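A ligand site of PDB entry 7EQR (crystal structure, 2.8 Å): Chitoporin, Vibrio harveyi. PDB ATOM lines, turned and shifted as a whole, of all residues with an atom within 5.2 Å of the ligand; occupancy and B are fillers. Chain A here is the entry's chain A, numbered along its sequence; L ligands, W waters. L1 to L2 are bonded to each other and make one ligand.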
ATOM      1  N   GLN A   9     -37.218   4.572  23.377  1.00  0.00           N
ATOM      2  CA  GLN A   9     -36.781   5.516  22.367  1.00  0.00           C
ATOM      3  C   GLN A   9     -38.014   5.981  21.608  1.00  0.00           C
ATOM      4  O   GLN A   9     -38.726   5.159  21.031  1.00  0.00           O
ATOM      5  CB  GLN A   9     -35.776   4.861  21.411  1.00  0.00           C
ATOM      6  CG  GLN A   9     -35.253   5.761  20.328  1.00  0.00           C
ATOM      7  CD  GLN A   9     -34.699   4.984  19.144  1.00  0.00           C
ATOM      8  OE1 GLN A   9     -34.981   3.799  18.979  1.00  0.00           O
ATOM      9  NE2 GLN A   9     -33.903   5.658  18.307  1.00  0.00           N
ATOM     10  N   GLU A  34     -37.265  -1.128  24.099  1.00  0.00           N
ATOM     11  CA  GLU A  34     -36.337  -2.231  24.124  1.00  0.00           C
ATOM     12  C   GLU A  34     -35.978  -2.615  25.543  1.00  0.00           C
ATOM     13  O   GLU A  34     -34.978  -3.287  25.761  1.00  0.00           O
ATOM     14  CB  GLU A  34     -35.090  -1.875  23.316  1.00  0.00           C
ATOM     15  CG  GLU A  34     -35.376  -1.800  21.831  1.00  0.00           C
ATOM     16  CD  GLU A  34     -34.245  -1.213  20.978  1.00  0.00           C
ATOM     17  OE1 GLU A  34     -33.326  -0.552  21.533  1.00  0.00           O
ATOM     18  OE2 GLU A  34     -34.290  -1.401  19.737  1.00  0.00           O
ATOM     19  N   ARG A  36     -35.844  -4.754  28.883  1.00  0.00           N
ATOM     20  CA  ARG A  36     -35.746  -6.204  29.001  1.00  0.00           C
ATOM     21  C   ARG A  36     -35.362  -6.572  30.432  1.00  0.00           C
ATOM     22  O   ARG A  36     -34.680  -5.819  31.128  1.00  0.00           O
ATOM     23  CB  ARG A  36     -34.731  -6.775  28.004  1.00  0.00           C
ATOM     24  CG  ARG A  36     -33.353  -6.136  28.099  1.00  0.00           C
ATOM     25  CD  ARG A  36     -32.865  -5.867  26.721  1.00  0.00           C
ATOM     26  NE  ARG A  36     -31.530  -5.293  26.675  1.00  0.00           N
ATOM     27  CZ  ARG A  36     -31.265  -4.112  26.137  1.00  0.00           C
ATOM     28  NH1 ARG A  36     -32.258  -3.400  25.638  1.00  0.00           N
ATOM     29  NH2 ARG A  36     -30.029  -3.638  26.097  1.00  0.00           N
ATOM     30  N   TYR A  60     -36.862  -7.525  23.940  1.00  0.00           N
ATOM     31  CA  TYR A  60     -37.472  -6.196  23.971  1.00  0.00           C
ATOM     32  C   TYR A  60     -38.965  -6.313  24.233  1.00  0.00           C
ATOM     33  O   TYR A  60     -39.693  -6.972  23.481  1.00  0.00           O
ATOM     34  CB  TYR A  60     -37.243  -5.485  22.632  1.00  0.00           C
ATOM     35  CG  TYR A  60     -35.790  -5.239  22.272  1.00  0.00           C
ATOM     36  CD1 TYR A  60     -34.821  -5.184  23.259  1.00  0.00           C
ATOM     37  CD2 TYR A  60     -35.397  -5.061  20.940  1.00  0.00           C
ATOM     38  CE1 TYR A  60     -33.481  -4.960  22.933  1.00  0.00           C
ATOM     39  CE2 TYR A  60     -34.071  -4.839  20.603  1.00  0.00           C
ATOM     40  CZ  TYR A  60     -33.110  -4.791  21.609  1.00  0.00           C
ATOM     41  OH  TYR A  60     -31.778  -4.574  21.303  1.00  0.00           O
ATOM     42  N   ARG A  75     -33.035 -13.002  24.388  1.00  0.00           N
ATOM     43  CA  ARG A  75     -31.725 -12.404  24.259  1.00  0.00           C
ATOM     44  C   ARG A  75     -30.698 -13.359  24.868  1.00  0.00           C
ATOM     45  O   ARG A  75     -31.002 -14.524  25.121  1.00  0.00           O
ATOM     46  CB  ARG A  75     -31.737 -11.008  24.860  1.00  0.00           C
ATOM     47  CG  ARG A  75     -32.460 -10.040  23.930  1.00  0.00           C
ATOM     48  CD  ARG A  75     -32.569  -8.638  24.484  1.00  0.00           C
ATOM     49  NE  ARG A  75     -31.266  -8.004  24.635  1.00  0.00           N
ATOM     50  CZ  ARG A  75     -30.599  -7.438  23.631  1.00  0.00           C
ATOM     51  NH1 ARG A  75     -31.129  -7.452  22.402  1.00  0.00           N
ATOM     52  NH2 ARG A  75     -29.416  -6.874  23.856  1.00  0.00           N
ATOM     53  N   TYR A  99     -20.501 -10.747  15.077  1.00  0.00           N
ATOM     54  CA  TYR A  99     -21.627  -9.851  15.286  1.00  0.00           C
ATOM     55  C   TYR A  99     -21.346  -8.902  16.431  1.00  0.00           C
ATOM     56  O   TYR A  99     -21.666  -7.710  16.334  1.00  0.00           O
ATOM     57  CB  TYR A  99     -22.909 -10.633  15.552  1.00  0.00           C
ATOM     58  CG  TYR A  99     -24.047  -9.660  15.738  1.00  0.00           C
ATOM     59  CD1 TYR A  99     -24.488  -8.888  14.663  1.00  0.00           C
ATOM     60  CD2 TYR A  99     -24.602  -9.435  16.977  1.00  0.00           C
ATOM     61  CE1 TYR A  99     -25.486  -7.954  14.829  1.00  0.00           C
ATOM     62  CE2 TYR A  99     -25.608  -8.481  17.142  1.00  0.00           C
ATOM     63  CZ  TYR A  99     -26.046  -7.751  16.058  1.00  0.00           C
ATOM     64  OH  TYR A  99     -27.036  -6.810  16.214  1.00  0.00           O
ATOM     65  N   ASP A 103     -21.910  -5.039  15.940  1.00  0.00           N
ATOM     66  CA  ASP A 103     -22.877  -4.308  16.756  1.00  0.00           C
ATOM     67  C   ASP A 103     -22.202  -3.197  17.542  1.00  0.00           C
ATOM     68  O   ASP A 103     -22.560  -2.024  17.404  1.00  0.00           O
ATOM     69  CB  ASP A 103     -23.608  -5.249  17.706  1.00  0.00           C
ATOM     70  CG  ASP A 103     -24.640  -4.516  18.537  1.00  0.00           C
ATOM     71  OD1 ASP A 103     -25.649  -4.049  17.944  1.00  0.00           O
ATOM     72  OD2 ASP A 103     -24.429  -4.350  19.770  1.00  0.00           O
ATOM     73  N   TRP A 104     -21.242  -3.538  18.399  1.00  0.00           N
ATOM     74  CA  TRP A 104     -20.512  -2.525  19.121  1.00  0.00           C
ATOM     75  C   TRP A 104     -19.026  -2.637  18.814  1.00  0.00           C
ATOM     76  O   TRP A 104     -18.451  -3.730  18.915  1.00  0.00           O
ATOM     77  CB  TRP A 104     -20.733  -2.619  20.643  1.00  0.00           C
ATOM     78  CG  TRP A 104     -20.114  -1.472  21.374  1.00  0.00           C
ATOM     79  CD1 TRP A 104     -18.882  -1.432  21.938  1.00  0.00           C
ATOM     80  CD2 TRP A 104     -20.705  -0.177  21.608  1.00  0.00           C
ATOM     81  NE1 TRP A 104     -18.651  -0.202  22.510  1.00  0.00           N
ATOM     82  CE2 TRP A 104     -19.763   0.590  22.321  1.00  0.00           C
ATOM     83  CE3 TRP A 104     -21.933   0.402  21.277  1.00  0.00           C
ATOM     84  CZ2 TRP A 104     -20.011   1.904  22.718  1.00  0.00           C
ATOM     85  CZ3 TRP A 104     -22.181   1.716  21.673  1.00  0.00           C
ATOM     86  CH2 TRP A 104     -21.222   2.456  22.389  1.00  0.00           C
ATOM     87  N   ASN A 108     -23.447   1.672  16.314  1.00  0.00           N
ATOM     88  CA  ASN A 108     -23.993   2.796  17.047  1.00  0.00           C
ATOM     89  C   ASN A 108     -23.498   4.099  16.431  1.00  0.00           C
ATOM     90  O   ASN A 108     -22.308   4.226  16.118  1.00  0.00           O
ATOM     91  CB  ASN A 108     -23.564   2.731  18.502  1.00  0.00           C
ATOM     92  CG  ASN A 108     -24.359   3.655  19.374  1.00  0.00           C
ATOM     93  OD1 ASN A 108     -24.016   4.817  19.524  1.00  0.00           O
ATOM     94  ND2 ASN A 108     -25.440   3.141  19.927  1.00  0.00           N
ATOM     95  N   PRO A 109     -24.353   5.118  16.254  1.00  0.00           N
ATOM     96  CA  PRO A 109     -25.756   5.209  16.617  1.00  0.00           C
ATOM     97  C   PRO A 109     -26.666   5.137  15.394  1.00  0.00           C
ATOM     98  O   PRO A 109     -26.555   6.025  14.544  1.00  0.00           O
ATOM     99  CB  PRO A 109     -25.840   6.601  17.233  1.00  0.00           C
ATOM    100  CG  PRO A 109     -24.813   7.406  16.387  1.00  0.00           C
ATOM    101  CD  PRO A 109     -23.875   6.394  15.718  1.00  0.00           C
ATOM    102  N   TRP A 117     -27.666  -5.499   9.747  1.00  0.00           N
ATOM    103  CA  TRP A 117     -28.386  -6.397   8.851  1.00  0.00           C
ATOM    104  C   TRP A 117     -28.450  -5.869   7.418  1.00  0.00           C
ATOM    105  O   TRP A 117     -28.990  -6.552   6.548  1.00  0.00           O
ATOM    106  CB  TRP A 117     -29.805  -6.677   9.374  1.00  0.00           C
ATOM    107  CG  TRP A 117     -30.703  -5.446   9.488  1.00  0.00           C
ATOM    108  CD1 TRP A 117     -31.618  -5.011   8.581  1.00  0.00           C
ATOM    109  CD2 TRP A 117     -30.752  -4.518  10.581  1.00  0.00           C
ATOM    110  NE1 TRP A 117     -32.233  -3.860   9.028  1.00  0.00           N
ATOM    111  CE2 TRP A 117     -31.715  -3.535  10.257  1.00  0.00           C
ATOM    112  CE3 TRP A 117     -30.071  -4.423  11.788  1.00  0.00           C
ATOM    113  CZ2 TRP A 117     -32.013  -2.480  11.099  1.00  0.00           C
ATOM    114  CZ3 TRP A 117     -30.364  -3.359  12.640  1.00  0.00           C
ATOM    115  CH2 TRP A 117     -31.336  -2.406  12.286  1.00  0.00           C
ATOM    116  N   GLN A 279     -25.698  12.440  17.054  1.00  0.00           N
ATOM    117  CA  GLN A 279     -26.256  12.064  18.341  1.00  0.00           C
ATOM    118  C   GLN A 279     -25.637  12.897  19.452  1.00  0.00           C
ATOM    119  O   GLN A 279     -24.414  12.984  19.563  1.00  0.00           O
ATOM    120  CB  GLN A 279     -26.040  10.573  18.649  1.00  0.00           C
ATOM    121  CG  GLN A 279     -26.743  10.134  19.938  1.00  0.00           C
ATOM    122  CD  GLN A 279     -26.447   8.704  20.370  1.00  0.00           C
ATOM    123  OE1 GLN A 279     -27.156   7.782  19.987  1.00  0.00           O
ATOM    124  NE2 GLN A 279     -25.406   8.532  21.198  1.00  0.00           N
ATOM    125  N   MET A 281     -25.767  13.094  23.669  1.00  0.00           N
ATOM    126  CA  MET A 281     -26.113  12.203  24.764  1.00  0.00           C
ATOM    127  C   MET A 281     -25.749  12.852  26.094  1.00  0.00           C
ATOM    128  O   MET A 281     -24.684  13.453  26.229  1.00  0.00           O
ATOM    129  CB  MET A 281     -25.398  10.865  24.641  1.00  0.00           C
ATOM    130  CG  MET A 281     -25.490  10.027  25.902  1.00  0.00           C
ATOM    131  SD  MET A 281     -24.781   8.368  25.747  1.00  0.00           S
ATOM    132  CE  MET A 281     -25.176   7.952  24.048  1.00  0.00           C
ATOM    133  N   VAL A 289     -28.741   7.229  30.755  1.00  0.00           N
ATOM    134  CA  VAL A 289     -28.383   8.239  29.768  1.00  0.00           C
ATOM    135  C   VAL A 289     -29.669   8.745  29.124  1.00  0.00           C
ATOM    136  O   VAL A 289     -30.662   8.016  29.028  1.00  0.00           O
ATOM    137  CB  VAL A 289     -27.435   7.688  28.685  1.00  0.00           C
ATOM    138  CG1 VAL A 289     -26.107   7.319  29.287  1.00  0.00           C
ATOM    139  CG2 VAL A 289     -28.052   6.474  28.026  1.00  0.00           C
ATOM    140  N   TYR A 291     -30.724  10.851  25.322  1.00  0.00           N
ATOM    141  CA  TYR A 291     -30.070  11.094  24.036  1.00  0.00           C
ATOM    142  C   TYR A 291     -31.066  11.524  22.973  1.00  0.00           C
ATOM    143  O   TYR A 291     -32.195  11.028  22.921  1.00  0.00           O
ATOM    144  CB  TYR A 291     -29.296   9.862  23.552  1.00  0.00           C
ATOM    145  CG  TYR A 291     -30.140   8.660  23.179  1.00  0.00           C
ATOM    146  CD1 TYR A 291     -30.678   8.537  21.892  1.00  0.00           C
ATOM    147  CD2 TYR A 291     -30.393   7.642  24.083  1.00  0.00           C
ATOM    148  CE1 TYR A 291     -31.432   7.443  21.542  1.00  0.00           C
ATOM    149  CE2 TYR A 291     -31.154   6.540  23.742  1.00  0.00           C
ATOM    150  CZ  TYR A 291     -31.674   6.440  22.466  1.00  0.00           C
ATOM    151  OH  TYR A 291     -32.442   5.344  22.115  1.00  0.00           O
ATOM    152  N   ARG A 293     -31.070  11.929  18.619  1.00  0.00           N
ATOM    153  CA  ARG A 293     -30.378  11.335  17.490  1.00  0.00           C
ATOM    154  C   ARG A 293     -31.132  11.657  16.216  1.00  0.00           C
ATOM    155  O   ARG A 293     -32.370  11.620  16.173  1.00  0.00           O
ATOM    156  CB  ARG A 293     -30.238   9.820  17.684  1.00  0.00           C
ATOM    157  CG  ARG A 293     -29.630   9.062  16.524  1.00  0.00           C
ATOM    158  CD  ARG A 293     -29.586   7.535  16.791  1.00  0.00           C
ATOM    159  NE  ARG A 293     -29.142   7.198  18.145  1.00  0.00           N
ATOM    160  CZ  ARG A 293     -29.250   5.988  18.714  1.00  0.00           C
ATOM    161  NH1 ARG A 293     -29.784   4.978  18.045  1.00  0.00           N
ATOM    162  NH2 ARG A 293     -28.818   5.795  19.952  1.00  0.00           N
ATOM    163  N   GLU A 328     -32.048   5.359  28.659  1.00  0.00           N
ATOM    164  CA  GLU A 328     -31.620   3.991  28.948  1.00  0.00           C
ATOM    165  C   GLU A 328     -31.080   3.912  30.361  1.00  0.00           C
ATOM    166  O   GLU A 328     -30.217   4.690  30.748  1.00  0.00           O
ATOM    167  CB  GLU A 328     -30.556   3.510  27.971  1.00  0.00           C
ATOM    168  CG  GLU A 328     -31.148   2.867  26.746  1.00  0.00           C
ATOM    169  CD  GLU A 328     -30.094   2.288  25.822  1.00  0.00           C
ATOM    170  OE1 GLU A 328     -28.969   1.962  26.309  1.00  0.00           O
ATOM    171  OE2 GLU A 328     -30.389   2.166  24.612  1.00  0.00           O
ATOM    172  N   TYR A 330     -29.772   1.181  33.366  1.00  0.00           N
ATOM    173  CA  TYR A 330     -29.285  -0.146  33.678  1.00  0.00           C
ATOM    174  C   TYR A 330     -29.435  -0.391  35.179  1.00  0.00           C
ATOM    175  O   TYR A 330     -29.141   0.491  35.986  1.00  0.00           O
ATOM    176  CB  TYR A 330     -27.837  -0.300  33.249  1.00  0.00           C
ATOM    177  CG  TYR A 330     -27.592   0.124  31.810  1.00  0.00           C
ATOM    178  CD1 TYR A 330     -27.525   1.481  31.464  1.00  0.00           C
ATOM    179  CD2 TYR A 330     -27.412  -0.812  30.776  1.00  0.00           C
ATOM    180  CE1 TYR A 330     -27.288   1.894  30.145  1.00  0.00           C
ATOM    181  CE2 TYR A 330     -27.180  -0.406  29.447  1.00  0.00           C
ATOM    182  CZ  TYR A 330     -27.123   0.958  29.140  1.00  0.00           C
ATOM    183  OH  TYR A 330     -26.890   1.400  27.840  1.00  0.00           O
HETATM  184  C1  LIG L   1     -25.039   1.809  23.833  1.00  0.00           C
HETATM  185  C2  LIG L   1     -26.272   2.365  23.071  1.00  0.00           C
HETATM  186  C3  LIG L   1     -27.355   1.294  22.928  1.00  0.00           C
HETATM  187  C4  LIG L   1     -26.739  -0.015  22.446  1.00  0.00           C
HETATM  188  C5  LIG L   1     -25.719  -0.529  23.473  1.00  0.00           C
HETATM  189  C6  LIG L   1     -24.440  -1.045  22.833  1.00  0.00           C
HETATM  190  C7  LIG L   1     -26.868   4.732  23.113  1.00  0.00           C
HETATM  191  C8  LIG L   1     -27.481   5.846  23.902  1.00  0.00           C
HETATM  192  N1  LIG L   1     -26.817   3.543  23.712  1.00  0.00           N
HETATM  193  O1  LIG L   1     -28.359   1.765  22.034  1.00  0.00           O
HETATM  194  O2  LIG L   1     -27.752  -1.001  22.326  1.00  0.00           O
HETATM  195  O3  LIG L   1     -25.332   0.506  24.402  1.00  0.00           O
HETATM  196  O4  LIG L   1     -23.980  -2.228  23.490  1.00  0.00           O
HETATM  197  O5  LIG L   1     -26.439   4.912  21.974  1.00  0.00           O
HETATM  198  C1  LG2 L   2     -28.103  -1.176  20.953  1.00  0.00           C
HETATM  199  C2  LG2 L   2     -28.459  -2.652  20.761  1.00  0.00           C
HETATM  200  C3  LG2 L   2     -28.897  -2.921  19.315  1.00  0.00           C
HETATM  201  C4  LG2 L   2     -30.066  -1.998  18.958  1.00  0.00           C
HETATM  202  C5  LG2 L   2     -29.630  -0.536  19.156  1.00  0.00           C
HETATM  203  C6  LG2 L   2     -30.705   0.489  18.853  1.00  0.00           C
HETATM  204  C7  LG2 L   2     -27.171  -3.975  22.411  1.00  0.00           C
HETATM  205  C8  LG2 L   2     -28.203  -3.562  23.422  1.00  0.00           C
HETATM  206  N1  LG2 L   2     -27.347  -3.515  21.152  1.00  0.00           N
HETATM  207  O1  LG2 L   2     -29.213  -4.301  19.143  1.00  0.00           O
HETATM  208  O2  LG2 L   2     -30.582  -2.190  17.645  1.00  0.00           O
HETATM  209  O3  LG2 L   2     -29.225  -0.343  20.532  1.00  0.00           O
HETATM  210  O4  LG2 L   2     -30.343   1.796  19.291  1.00  0.00           O
HETATM  211  O5  LG2 L   2     -26.222  -4.698  22.717  1.00  0.00           O
HETATM  212  O   HOH W   1     -27.755   2.047  17.675  1.00  0.00           O
HETATM  213  O   HOH W   2     -25.874  -6.147  24.978  1.00  0.00           O
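OE1 of Glu 328 sits at hydrogen-bond distance from OH of Tyr 330. The side-chain hydroxyl (OH) of Tyr 60 lies within hydrogen-bond range of the guanidinium group (NH1) of Arg 75. The guanidinium group (NH1) of Arg 36 lies within hydrogen-bond range of the backbone carbonyl oxygen (O) of Glu 34, at 2.7 Å. O of Glu 328 is in hydrogen-bond range of N of Val 289 (2.9 Å). The guanidinium group (NH2) of Arg 293 sits at hydrogen-bond distance from the side-chain amide oxygen (OE1) of Gln 279 (2.6 Å).
OH of Tyr 60 sits at hydrogen-bond distance from O1 of LG2 L2 (3.4 Å). The side-chain amide nitrogen (ND2) of Asn 108 sits at hydrogen-bond distance from an oxygen (O5) of LIG L1 (2.9 Å). OE2 of Glu 328 sits at hydrogen-bond distance from O1 of LIG L1 (3.3 Å). The guanidinium group (NH2) of Arg 293 lies within hydrogen-bond range of an oxygen (O5) of LIG L1 (3.2 Å). A nitrogen (N1) of LG2 L2 sits at hydrogen-bond distance from the side-chain carboxylate of Asp 103 (3.3 Å).
Merely in contact with the ligand: Glu 34, Arg 36, Arg 75, Trp 104, Gln 279, Met 281, Tyr 291 and Tyr 330. Hydrophobic or aromatic side chains that line the ligand: Trp 104, Met 281 and Tyr 291. Within 4 Å of the ligand: Glu 34, Arg 36, Tyr 60, Arg 75, Asp 103, Trp 104, Asn 108, Gln 279, Met 281, Tyr 291, Arg 293, Glu 328 and Tyr 330. The nearest printed residue that does not touch the ligand is Val 289 (4.2 Å).
Water W1 bridges an oxygen (O4) of LG2 L2 and the side-chain amide nitrogen (ND2) of Asn 108.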
